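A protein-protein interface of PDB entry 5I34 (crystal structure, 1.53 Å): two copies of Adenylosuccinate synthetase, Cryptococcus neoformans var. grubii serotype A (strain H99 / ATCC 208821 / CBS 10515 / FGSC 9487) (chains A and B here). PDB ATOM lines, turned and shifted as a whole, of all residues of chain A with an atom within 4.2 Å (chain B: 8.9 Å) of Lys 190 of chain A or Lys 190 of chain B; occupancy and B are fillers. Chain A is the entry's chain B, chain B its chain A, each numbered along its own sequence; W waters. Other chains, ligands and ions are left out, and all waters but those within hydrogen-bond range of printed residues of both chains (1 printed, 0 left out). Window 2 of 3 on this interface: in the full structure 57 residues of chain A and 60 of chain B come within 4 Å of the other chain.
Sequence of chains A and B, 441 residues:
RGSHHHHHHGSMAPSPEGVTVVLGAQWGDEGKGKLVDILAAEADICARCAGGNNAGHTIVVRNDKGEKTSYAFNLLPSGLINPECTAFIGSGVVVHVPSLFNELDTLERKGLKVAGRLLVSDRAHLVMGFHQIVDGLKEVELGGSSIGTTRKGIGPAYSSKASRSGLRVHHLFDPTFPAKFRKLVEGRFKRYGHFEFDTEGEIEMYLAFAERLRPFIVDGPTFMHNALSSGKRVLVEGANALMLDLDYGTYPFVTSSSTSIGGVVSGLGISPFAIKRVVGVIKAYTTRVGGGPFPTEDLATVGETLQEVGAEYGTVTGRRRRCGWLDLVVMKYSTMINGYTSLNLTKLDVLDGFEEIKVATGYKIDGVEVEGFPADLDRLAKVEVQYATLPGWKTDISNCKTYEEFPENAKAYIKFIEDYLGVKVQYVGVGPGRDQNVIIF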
ATOM      1  N   GLU A 186       1.787 -22.369 -22.452  1.00  0.00           N
ATOM      2  CA  GLU A 186       1.930 -21.025 -22.987  1.00  0.00           C
ATOM      3  C   GLU A 186       3.406 -20.660 -23.138  1.00  0.00           C
ATOM      4  O   GLU A 186       3.810 -20.082 -24.153  1.00  0.00           O
ATOM      5  CB  GLU A 186       1.216 -20.031 -22.080  1.00  0.00           C
ATOM      6  CG  GLU A 186       1.223 -18.607 -22.582  1.00  0.00           C
ATOM      7  CD  GLU A 186       0.541 -17.651 -21.616  1.00  0.00           C
ATOM      8  OE1 GLU A 186       1.226 -16.751 -21.096  1.00  0.00           O
ATOM      9  OE2 GLU A 186      -0.676 -17.798 -21.371  1.00  0.00           O
ATOM     10  N   GLY A 187       4.216 -21.034 -22.144  1.00  0.00           N
ATOM     11  CA  GLY A 187       5.649 -20.781 -22.184  1.00  0.00           C
ATOM     12  C   GLY A 187       6.353 -21.536 -23.304  1.00  0.00           C
ATOM     13  O   GLY A 187       7.253 -21.007 -23.959  1.00  0.00           O
ATOM     14  N   ARG A 188       5.956 -22.787 -23.529  1.00  0.00           N
ATOM     15  CA  ARG A 188       6.523 -23.555 -24.632  1.00  0.00           C
ATOM     16  C   ARG A 188       6.137 -22.940 -25.995  1.00  0.00           C
ATOM     17  O   ARG A 188       6.938 -22.940 -26.939  1.00  0.00           O
ATOM     18  CB  ARG A 188       6.068 -25.019 -24.564  1.00  0.00           C
ATOM     19  CG  ARG A 188       6.507 -25.794 -23.292  1.00  0.00           C
ATOM     20  CD  ARG A 188       8.019 -25.733 -23.039  1.00  0.00           C
ATOM     21  NE  ARG A 188       8.394 -24.512 -22.336  1.00  0.00           N
ATOM     22  CZ  ARG A 188       9.585 -23.921 -22.388  1.00  0.00           C
ATOM     23  NH1 ARG A 188      10.568 -24.422 -23.129  1.00  0.00           N
ATOM     24  NH2 ARG A 188       9.778 -22.803 -21.696  1.00  0.00           N
ATOM     25  N   PHE A 189       4.913 -22.448 -26.121  1.00  0.00           N
ATOM     26  CA  PHE A 189       4.506 -21.747 -27.351  1.00  0.00           C
ATOM     27  C   PHE A 189       5.382 -20.523 -27.597  1.00  0.00           C
ATOM     28  O   PHE A 189       5.761 -20.244 -28.741  1.00  0.00           O
ATOM     29  CB  PHE A 189       3.035 -21.317 -27.293  1.00  0.00           C
ATOM     30  CG  PHE A 189       2.044 -22.456 -27.394  1.00  0.00           C
ATOM     31  CD1 PHE A 189       2.379 -23.656 -28.009  1.00  0.00           C
ATOM     32  CD2 PHE A 189       0.765 -22.315 -26.872  1.00  0.00           C
ATOM     33  CE1 PHE A 189       1.462 -24.697 -28.093  1.00  0.00           C
ATOM     34  CE2 PHE A 189      -0.155 -23.346 -26.953  1.00  0.00           C
ATOM     35  CZ  PHE A 189       0.196 -24.545 -27.567  1.00  0.00           C
ATOM     36  N   LYS A 190       5.699 -19.774 -26.541  1.00  0.00           N
ATOM     37  CA  LYS A 190       6.574 -18.612 -26.697  1.00  0.00           C
ATOM     38  C   LYS A 190       7.920 -19.032 -27.259  1.00  0.00           C
ATOM     39  O   LYS A 190       8.433 -18.417 -28.189  1.00  0.00           O
ATOM     40  CB  LYS A 190       6.764 -17.884 -25.361  1.00  0.00           C
ATOM     41  CG  LYS A 190       5.528 -17.143 -24.874  1.00  0.00           C
ATOM     42  CD  LYS A 190       5.780 -16.469 -23.521  1.00  0.00           C
ATOM     43  CE  LYS A 190       4.503 -15.885 -22.924  1.00  0.00           C
ATOM     44  NZ  LYS A 190       3.879 -14.909 -23.820  1.00  0.00           N
ATOM     45  N   ARG A 191       8.492 -20.079 -26.682  1.00  0.00           N
ATOM     46  CA  ARG A 191       9.845 -20.507 -27.028  1.00  0.00           C
ATOM     47  C   ARG A 191       9.926 -21.168 -28.398  1.00  0.00           C
ATOM     48  O   ARG A 191      10.872 -20.921 -29.148  1.00  0.00           O
ATOM     49  CB  ARG A 191      10.369 -21.476 -25.973  1.00  0.00           C
ATOM     50  CG  ARG A 191      11.709 -22.113 -26.303  1.00  0.00           C
ATOM     51  CD  ARG A 191      12.790 -21.075 -26.432  1.00  0.00           C
ATOM     52  NE  ARG A 191      14.074 -21.697 -26.727  1.00  0.00           N
ATOM     53  CZ  ARG A 191      14.449 -22.074 -27.944  1.00  0.00           C
ATOM     54  NH1 ARG A 191      13.633 -21.895 -28.977  1.00  0.00           N
ATOM     55  NH2 ARG A 191      15.636 -22.638 -28.128  1.00  0.00           N
ATOM     56  N   TYR A 192       8.950 -22.014 -28.716  1.00  0.00           N
ATOM     57  CA  TYR A 192       9.050 -22.871 -29.894  1.00  0.00           C
ATOM     58  C   TYR A 192       8.025 -22.548 -30.976  1.00  0.00           C
ATOM     59  O   TYR A 192       8.038 -23.152 -32.058  1.00  0.00           O
ATOM     60  CB  TYR A 192       8.917 -24.337 -29.468  1.00  0.00           C
ATOM     61  CG  TYR A 192      10.117 -24.826 -28.687  1.00  0.00           C
ATOM     62  CD1 TYR A 192      11.350 -25.015 -29.307  1.00  0.00           C
ATOM     63  CD2 TYR A 192      10.026 -25.096 -27.330  1.00  0.00           C
ATOM     64  CE1 TYR A 192      12.454 -25.459 -28.586  1.00  0.00           C
ATOM     65  CE2 TYR A 192      11.116 -25.536 -26.614  1.00  0.00           C
ATOM     66  CZ  TYR A 192      12.328 -25.718 -27.242  1.00  0.00           C
ATOM     67  OH  TYR A 192      13.406 -26.161 -26.505  1.00  0.00           O
ATOM     68  N   VAL B 134      17.062 -12.929 -17.074  1.00  0.00           N
ATOM     69  CA  VAL B 134      15.810 -13.659 -17.230  1.00  0.00           C
ATOM     70  C   VAL B 134      15.330 -14.239 -15.886  1.00  0.00           C
ATOM     71  O   VAL B 134      14.141 -14.528 -15.744  1.00  0.00           O
ATOM     72  CB  VAL B 134      15.898 -14.772 -18.289  1.00  0.00           C
ATOM     73  CG1 VAL B 134      16.273 -14.186 -19.624  1.00  0.00           C
ATOM     74  CG2 VAL B 134      16.877 -15.842 -17.912  1.00  0.00           C
ATOM     75  N   LYS B 138      11.461 -13.718 -15.165  1.00  0.00           N
ATOM     76  CA  LYS B 138      10.577 -14.814 -14.787  1.00  0.00           C
ATOM     77  C   LYS B 138       9.898 -14.507 -13.456  1.00  0.00           C
ATOM     78  O   LYS B 138       8.696 -14.723 -13.276  1.00  0.00           O
ATOM     79  CB  LYS B 138      11.375 -16.124 -14.713  1.00  0.00           C
ATOM     80  CG  LYS B 138      10.605 -17.330 -14.217  1.00  0.00           C
ATOM     81  CD  LYS B 138       9.391 -17.615 -15.068  1.00  0.00           C
ATOM     82  CE  LYS B 138       8.585 -18.767 -14.498  1.00  0.00           C
ATOM     83  NZ  LYS B 138       7.278 -18.892 -15.186  1.00  0.00           N
ATOM     84  N   GLU B 141       7.241 -12.059 -14.073  1.00  0.00           N
ATOM     85  CA  GLU B 141       6.203 -12.806 -14.787  1.00  0.00           C
ATOM     86  C   GLU B 141       5.305 -13.623 -13.843  1.00  0.00           C
ATOM     87  O   GLU B 141       4.115 -13.826 -14.122  1.00  0.00           O
ATOM     88  CB  GLU B 141       6.883 -13.718 -15.813  1.00  0.00           C
ATOM     89  CG  GLU B 141       5.991 -14.323 -16.869  1.00  0.00           C
ATOM     90  CD  GLU B 141       6.797 -15.097 -17.891  1.00  0.00           C
ATOM     91  OE1 GLU B 141       6.925 -16.331 -17.745  1.00  0.00           O
ATOM     92  OE2 GLU B 141       7.329 -14.466 -18.830  1.00  0.00           O
ATOM     93  N   LYS B 183      23.423 -18.037 -29.913  1.00  0.00           N
ATOM     94  CA  LYS B 183      22.234 -18.874 -30.003  1.00  0.00           C
ATOM     95  C   LYS B 183      21.506 -18.952 -28.673  1.00  0.00           C
ATOM     96  O   LYS B 183      20.278 -18.972 -28.645  1.00  0.00           O
ATOM     97  CB  LYS B 183      22.579 -20.279 -30.486  1.00  0.00           C
ATOM     98  CG  LYS B 183      22.763 -20.404 -31.990  1.00  0.00           C
ATOM     99  CD  LYS B 183      21.518 -19.953 -32.740  1.00  0.00           C
ATOM    100  CE  LYS B 183      21.645 -20.172 -34.228  1.00  0.00           C
ATOM    101  NZ  LYS B 183      20.455 -19.632 -34.939  1.00  0.00           N
ATOM    102  N   LEU B 184      22.258 -18.996 -27.576  1.00  0.00           N
ATOM    103  CA  LEU B 184      21.649 -18.966 -26.245  1.00  0.00           C
ATOM    104  C   LEU B 184      20.852 -17.680 -26.015  1.00  0.00           C
ATOM    105  O   LEU B 184      19.728 -17.725 -25.509  1.00  0.00           O
ATOM    106  CB  LEU B 184      22.718 -19.107 -25.170  1.00  0.00           C
ATOM    107  CG  LEU B 184      23.118 -20.544 -24.885  1.00  0.00           C
ATOM    108  CD1 LEU B 184      24.394 -20.519 -24.082  1.00  0.00           C
ATOM    109  CD2 LEU B 184      22.005 -21.271 -24.110  1.00  0.00           C
ATOM    110  N   VAL B 185      21.429 -16.539 -26.383  1.00  0.00           N
ATOM    111  CA  VAL B 185      20.734 -15.255 -26.269  1.00  0.00           C
ATOM    112  C   VAL B 185      19.447 -15.306 -27.082  1.00  0.00           C
ATOM    113  O   VAL B 185      18.377 -14.878 -26.628  1.00  0.00           O
ATOM    114  CB  VAL B 185      21.612 -14.062 -26.769  1.00  0.00           C
ATOM    115  CG1 VAL B 185      20.807 -12.744 -26.794  1.00  0.00           C
ATOM    116  CG2 VAL B 185      22.848 -13.892 -25.907  1.00  0.00           C
ATOM    117  N   GLU B 186      19.556 -15.844 -28.294  1.00  0.00           N
ATOM    118  CA  GLU B 186      18.414 -15.890 -29.206  1.00  0.00           C
ATOM    119  C   GLU B 186      17.266 -16.719 -28.616  1.00  0.00           C
ATOM    120  O   GLU B 186      16.092 -16.357 -28.749  1.00  0.00           O
ATOM    121  CB  GLU B 186      18.838 -16.451 -30.554  1.00  0.00           C
ATOM    122  CG  GLU B 186      19.757 -15.516 -31.332  1.00  0.00           C
ATOM    123  CD  GLU B 186      20.297 -16.133 -32.613  1.00  0.00           C
ATOM    124  OE1 GLU B 186      19.641 -17.044 -33.175  1.00  0.00           O
ATOM    125  OE2 GLU B 186      21.382 -15.698 -33.066  1.00  0.00           O
ATOM    126  N   GLY B 187      17.607 -17.814 -27.952  1.00  0.00           N
ATOM    127  CA  GLY B 187      16.605 -18.645 -27.307  1.00  0.00           C
ATOM    128  C   GLY B 187      15.897 -17.938 -26.164  1.00  0.00           C
ATOM    129  O   GLY B 187      14.681 -18.077 -25.998  1.00  0.00           O
ATOM    130  N   ARG B 188      16.656 -17.194 -25.360  1.00  0.00           N
ATOM    131  CA  ARG B 188      16.069 -16.430 -24.270  1.00  0.00           C
ATOM    132  C   ARG B 188      15.176 -15.327 -24.838  1.00  0.00           C
ATOM    133  O   ARG B 188      14.130 -15.026 -24.274  1.00  0.00           O
ATOM    134  CB  ARG B 188      17.145 -15.823 -23.363  1.00  0.00           C
ATOM    135  CG  ARG B 188      18.027 -16.820 -22.606  1.00  0.00           C
ATOM    136  CD  ARG B 188      17.233 -17.827 -21.825  1.00  0.00           C
ATOM    137  NE  ARG B 188      16.817 -18.917 -22.685  1.00  0.00           N
ATOM    138  CZ  ARG B 188      15.724 -19.654 -22.509  1.00  0.00           C
ATOM    139  NH1 ARG B 188      14.932 -19.453 -21.465  1.00  0.00           N
ATOM    140  NH2 ARG B 188      15.428 -20.597 -23.398  1.00  0.00           N
ATOM    141  N   PHE B 189      15.585 -14.725 -25.948  1.00  0.00           N
ATOM    142  CA  PHE B 189      14.751 -13.708 -26.594  1.00  0.00           C
ATOM    143  C   PHE B 189      13.428 -14.310 -27.047  1.00  0.00           C
ATOM    144  O   PHE B 189      12.399 -13.654 -26.962  1.00  0.00           O
ATOM    145  CB  PHE B 189      15.457 -13.069 -27.806  1.00  0.00           C
ATOM    146  CG  PHE B 189      16.503 -12.023 -27.454  1.00  0.00           C
ATOM    147  CD1 PHE B 189      16.703 -11.583 -26.146  1.00  0.00           C
ATOM    148  CD2 PHE B 189      17.281 -11.467 -28.451  1.00  0.00           C
ATOM    149  CE1 PHE B 189      17.682 -10.624 -25.854  1.00  0.00           C
ATOM    150  CE2 PHE B 189      18.244 -10.517 -28.158  1.00  0.00           C
ATOM    151  CZ  PHE B 189      18.437 -10.095 -26.851  1.00  0.00           C
ATOM    152  N   LYS B 190      13.445 -15.543 -27.540  1.00  0.00           N
ATOM    153  CA  LYS B 190      12.202 -16.188 -27.950  1.00  0.00           C
ATOM    154  C   LYS B 190      11.275 -16.417 -26.758  1.00  0.00           C
ATOM    155  O   LYS B 190      10.070 -16.188 -26.837  1.00  0.00           O
ATOM    156  CB  LYS B 190      12.480 -17.512 -28.653  1.00  0.00           C
ATOM    157  CG  LYS B 190      13.041 -17.320 -30.045  1.00  0.00           C
ATOM    158  CD  LYS B 190      13.268 -18.634 -30.756  1.00  0.00           C
ATOM    159  CE  LYS B 190      13.904 -18.403 -32.114  1.00  0.00           C
ATOM    160  NZ  LYS B 190      13.145 -17.397 -32.911  1.00  0.00           N
ATOM    161  N   ARG B 191      11.842 -16.878 -25.650  1.00  0.00           N
ATOM    162  CA  ARG B 191      11.034 -17.186 -24.482  1.00  0.00           C
ATOM    163  C   ARG B 191      10.514 -15.944 -23.772  1.00  0.00           C
ATOM    164  O   ARG B 191       9.349 -15.906 -23.353  1.00  0.00           O
ATOM    165  CB  ARG B 191      11.835 -18.037 -23.498  1.00  0.00           C
ATOM    166  CG  ARG B 191      11.127 -18.317 -22.175  1.00  0.00           C
ATOM    167  CD  ARG B 191       9.739 -18.942 -22.355  1.00  0.00           C
ATOM    168  NE  ARG B 191       9.109 -19.136 -21.059  1.00  0.00           N
ATOM    169  CZ  ARG B 191       8.474 -18.188 -20.375  1.00  0.00           C
ATOM    170  NH1 ARG B 191       8.362 -16.958 -20.858  1.00  0.00           N
ATOM    171  NH2 ARG B 191       7.954 -18.475 -19.194  1.00  0.00           N
ATOM    172  N   TYR B 192      11.373 -14.934 -23.625  1.00  0.00           N
ATOM    173  CA  TYR B 192      11.057 -13.784 -22.764  1.00  0.00           C
ATOM    174  C   TYR B 192      10.845 -12.456 -23.485  1.00  0.00           C
ATOM    175  O   TYR B 192      10.409 -11.493 -22.855  1.00  0.00           O
ATOM    176  CB  TYR B 192      12.165 -13.617 -21.722  1.00  0.00           C
ATOM    177  CG  TYR B 192      12.151 -14.693 -20.671  1.00  0.00           C
ATOM    178  CD1 TYR B 192      11.183 -14.698 -19.671  1.00  0.00           C
ATOM    179  CD2 TYR B 192      13.108 -15.705 -20.665  1.00  0.00           C
ATOM    180  CE1 TYR B 192      11.161 -15.689 -18.704  1.00  0.00           C
ATOM    181  CE2 TYR B 192      13.095 -16.696 -19.703  1.00  0.00           C
ATOM    182  CZ  TYR B 192      12.125 -16.678 -18.723  1.00  0.00           C
ATOM    183  OH  TYR B 192      12.118 -17.667 -17.768  1.00  0.00           O
ATOM    184  N   GLY B 193      11.120 -12.410 -24.787  1.00  0.00           N
ATOM    185  CA  GLY B 193      11.119 -11.166 -25.554  1.00  0.00           C
ATOM    186  C   GLY B 193      12.507 -10.539 -25.556  1.00  0.00           C
ATOM    187  O   GLY B 193      13.382 -11.016 -24.836  1.00  0.00           O
ATOM    188  N   HIS B 194      12.715  -9.489 -26.355  1.00  0.00           N
ATOM    189  CA  HIS B 194      14.025  -8.839 -26.430  1.00  0.00           C
ATOM    190  C   HIS B 194      14.221  -7.961 -25.222  1.00  0.00           C
ATOM    191  O   HIS B 194      13.429  -7.054 -24.953  1.00  0.00           O
ATOM    192  CB  HIS B 194      14.195  -7.963 -27.681  1.00  0.00           C
ATOM    193  CG  HIS B 194      14.278  -8.711 -28.969  1.00  0.00           C
ATOM    194  ND1 HIS B 194      13.944 -10.041 -29.098  1.00  0.00           N
ATOM    195  CD2 HIS B 194      14.648  -8.291 -30.202  1.00  0.00           C
ATOM    196  CE1 HIS B 194      14.121 -10.410 -30.356  1.00  0.00           C
ATOM    197  NE2 HIS B 194      14.534  -9.367 -31.046  1.00  0.00           N
ATOM    198  N   PHE B 195      15.279  -8.230 -24.488  1.00  0.00           N
ATOM    199  CA  PHE B 195      15.738  -7.343 -23.444  1.00  0.00           C
ATOM    200  C   PHE B 195      17.069  -6.770 -23.890  1.00  0.00           C
ATOM    201  O   PHE B 195      17.736  -7.341 -24.761  1.00  0.00           O
ATOM    202  CB  PHE B 195      15.856  -8.090 -22.113  1.00  0.00           C
ATOM    203  CG  PHE B 195      16.536  -9.436 -22.219  1.00  0.00           C
ATOM    204  CD1 PHE B 195      15.799 -10.584 -22.482  1.00  0.00           C
ATOM    205  CD2 PHE B 195      17.909  -9.553 -22.065  1.00  0.00           C
ATOM    206  CE1 PHE B 195      16.435 -11.833 -22.574  1.00  0.00           C
ATOM    207  CE2 PHE B 195      18.542 -10.794 -22.162  1.00  0.00           C
ATOM    208  CZ  PHE B 195      17.802 -11.926 -22.416  1.00  0.00           C
HETATM  209  O   HOH W   1       8.742 -16.054 -29.387  1.00  0.00           O
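O of Lys 190 of chain A lies close to O of Lys 190 of chain B.
NH2 of Arg 191 of chain B lies within salt-bridge range of OE1 of Glu 141 of chain B.
Among the printed residues, pairs that only touch across the chains: Gly 187 of chain A with Arg 191 of chain B, Arg 188 of chain A with Arg 191 of chain B, Lys 190 of chain A with Arg 191 of chain B, Arg 191 of chain A with Gly 187 of chain B, Arg 191 of chain A with Arg 188 of chain B and Arg 191 of chain A with Lys 190 of chain B.
Lys 190 of chain A touches two residues of chain B.
Of the printed residues of chain B, Arg 191 of chain A touches Gly 187 (3.6 Å), Arg 188 (3.8 Å) and Lys 190 (3.7 Å).
Printed residues of chain A within 4 Å of Gly 187 of chain B: Arg 191 (3.6 Å).
Lys 190 of chain B touches two residues of chain A.
Phe 195 of chain B touches none of the printed residues of chain A.
The nearest residue of chain B that does not touch Lys 190 of chain A is Glu 141 of chain B (5.2 Å).
Of the 7 printed residues of chain A, 4 touch a printed residue of chain B.
Along chain A the printed residues that touch a printed residue of chain B span positions 187 to 191.
Of the 16 printed residues of chain B, 4 touch a printed residue of chain A.
Among the printed residues, 7 pairs touch across the chains.
Among the printed residues, no Asp or Glu carboxylate lies within 4 Å of a Lys or Arg side-chain nitrogen of the other chain.
Gly 187 of chain A touches Arg 191 of chain B, and with the chains exchanged Arg 191 of chain A touches Gly 187 of chain B.
Arg 188 of chain A touches Arg 191 of chain B, and with the chains exchanged Arg 191 of chain A touches Arg 188 of chain B.
Lys 190 of chain B touches its own counterpart, Lys 190 of chain A.
Lys 190 of chain A touches Arg 191 of chain B, and with the chains exchanged Arg 191 of chain A touches Lys 190 of chain B.
Of the 7 pairs that touch across the chains among the printed residues, 7 have their exchanged pair printed and touching as well.
Water W1 bridges the backbone carbonyl oxygen (O) of Lys 190 of chain A (2.7 Å) and the backbone carbonyl oxygen (O) of Lys 190 of chain B (2.9 Å).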
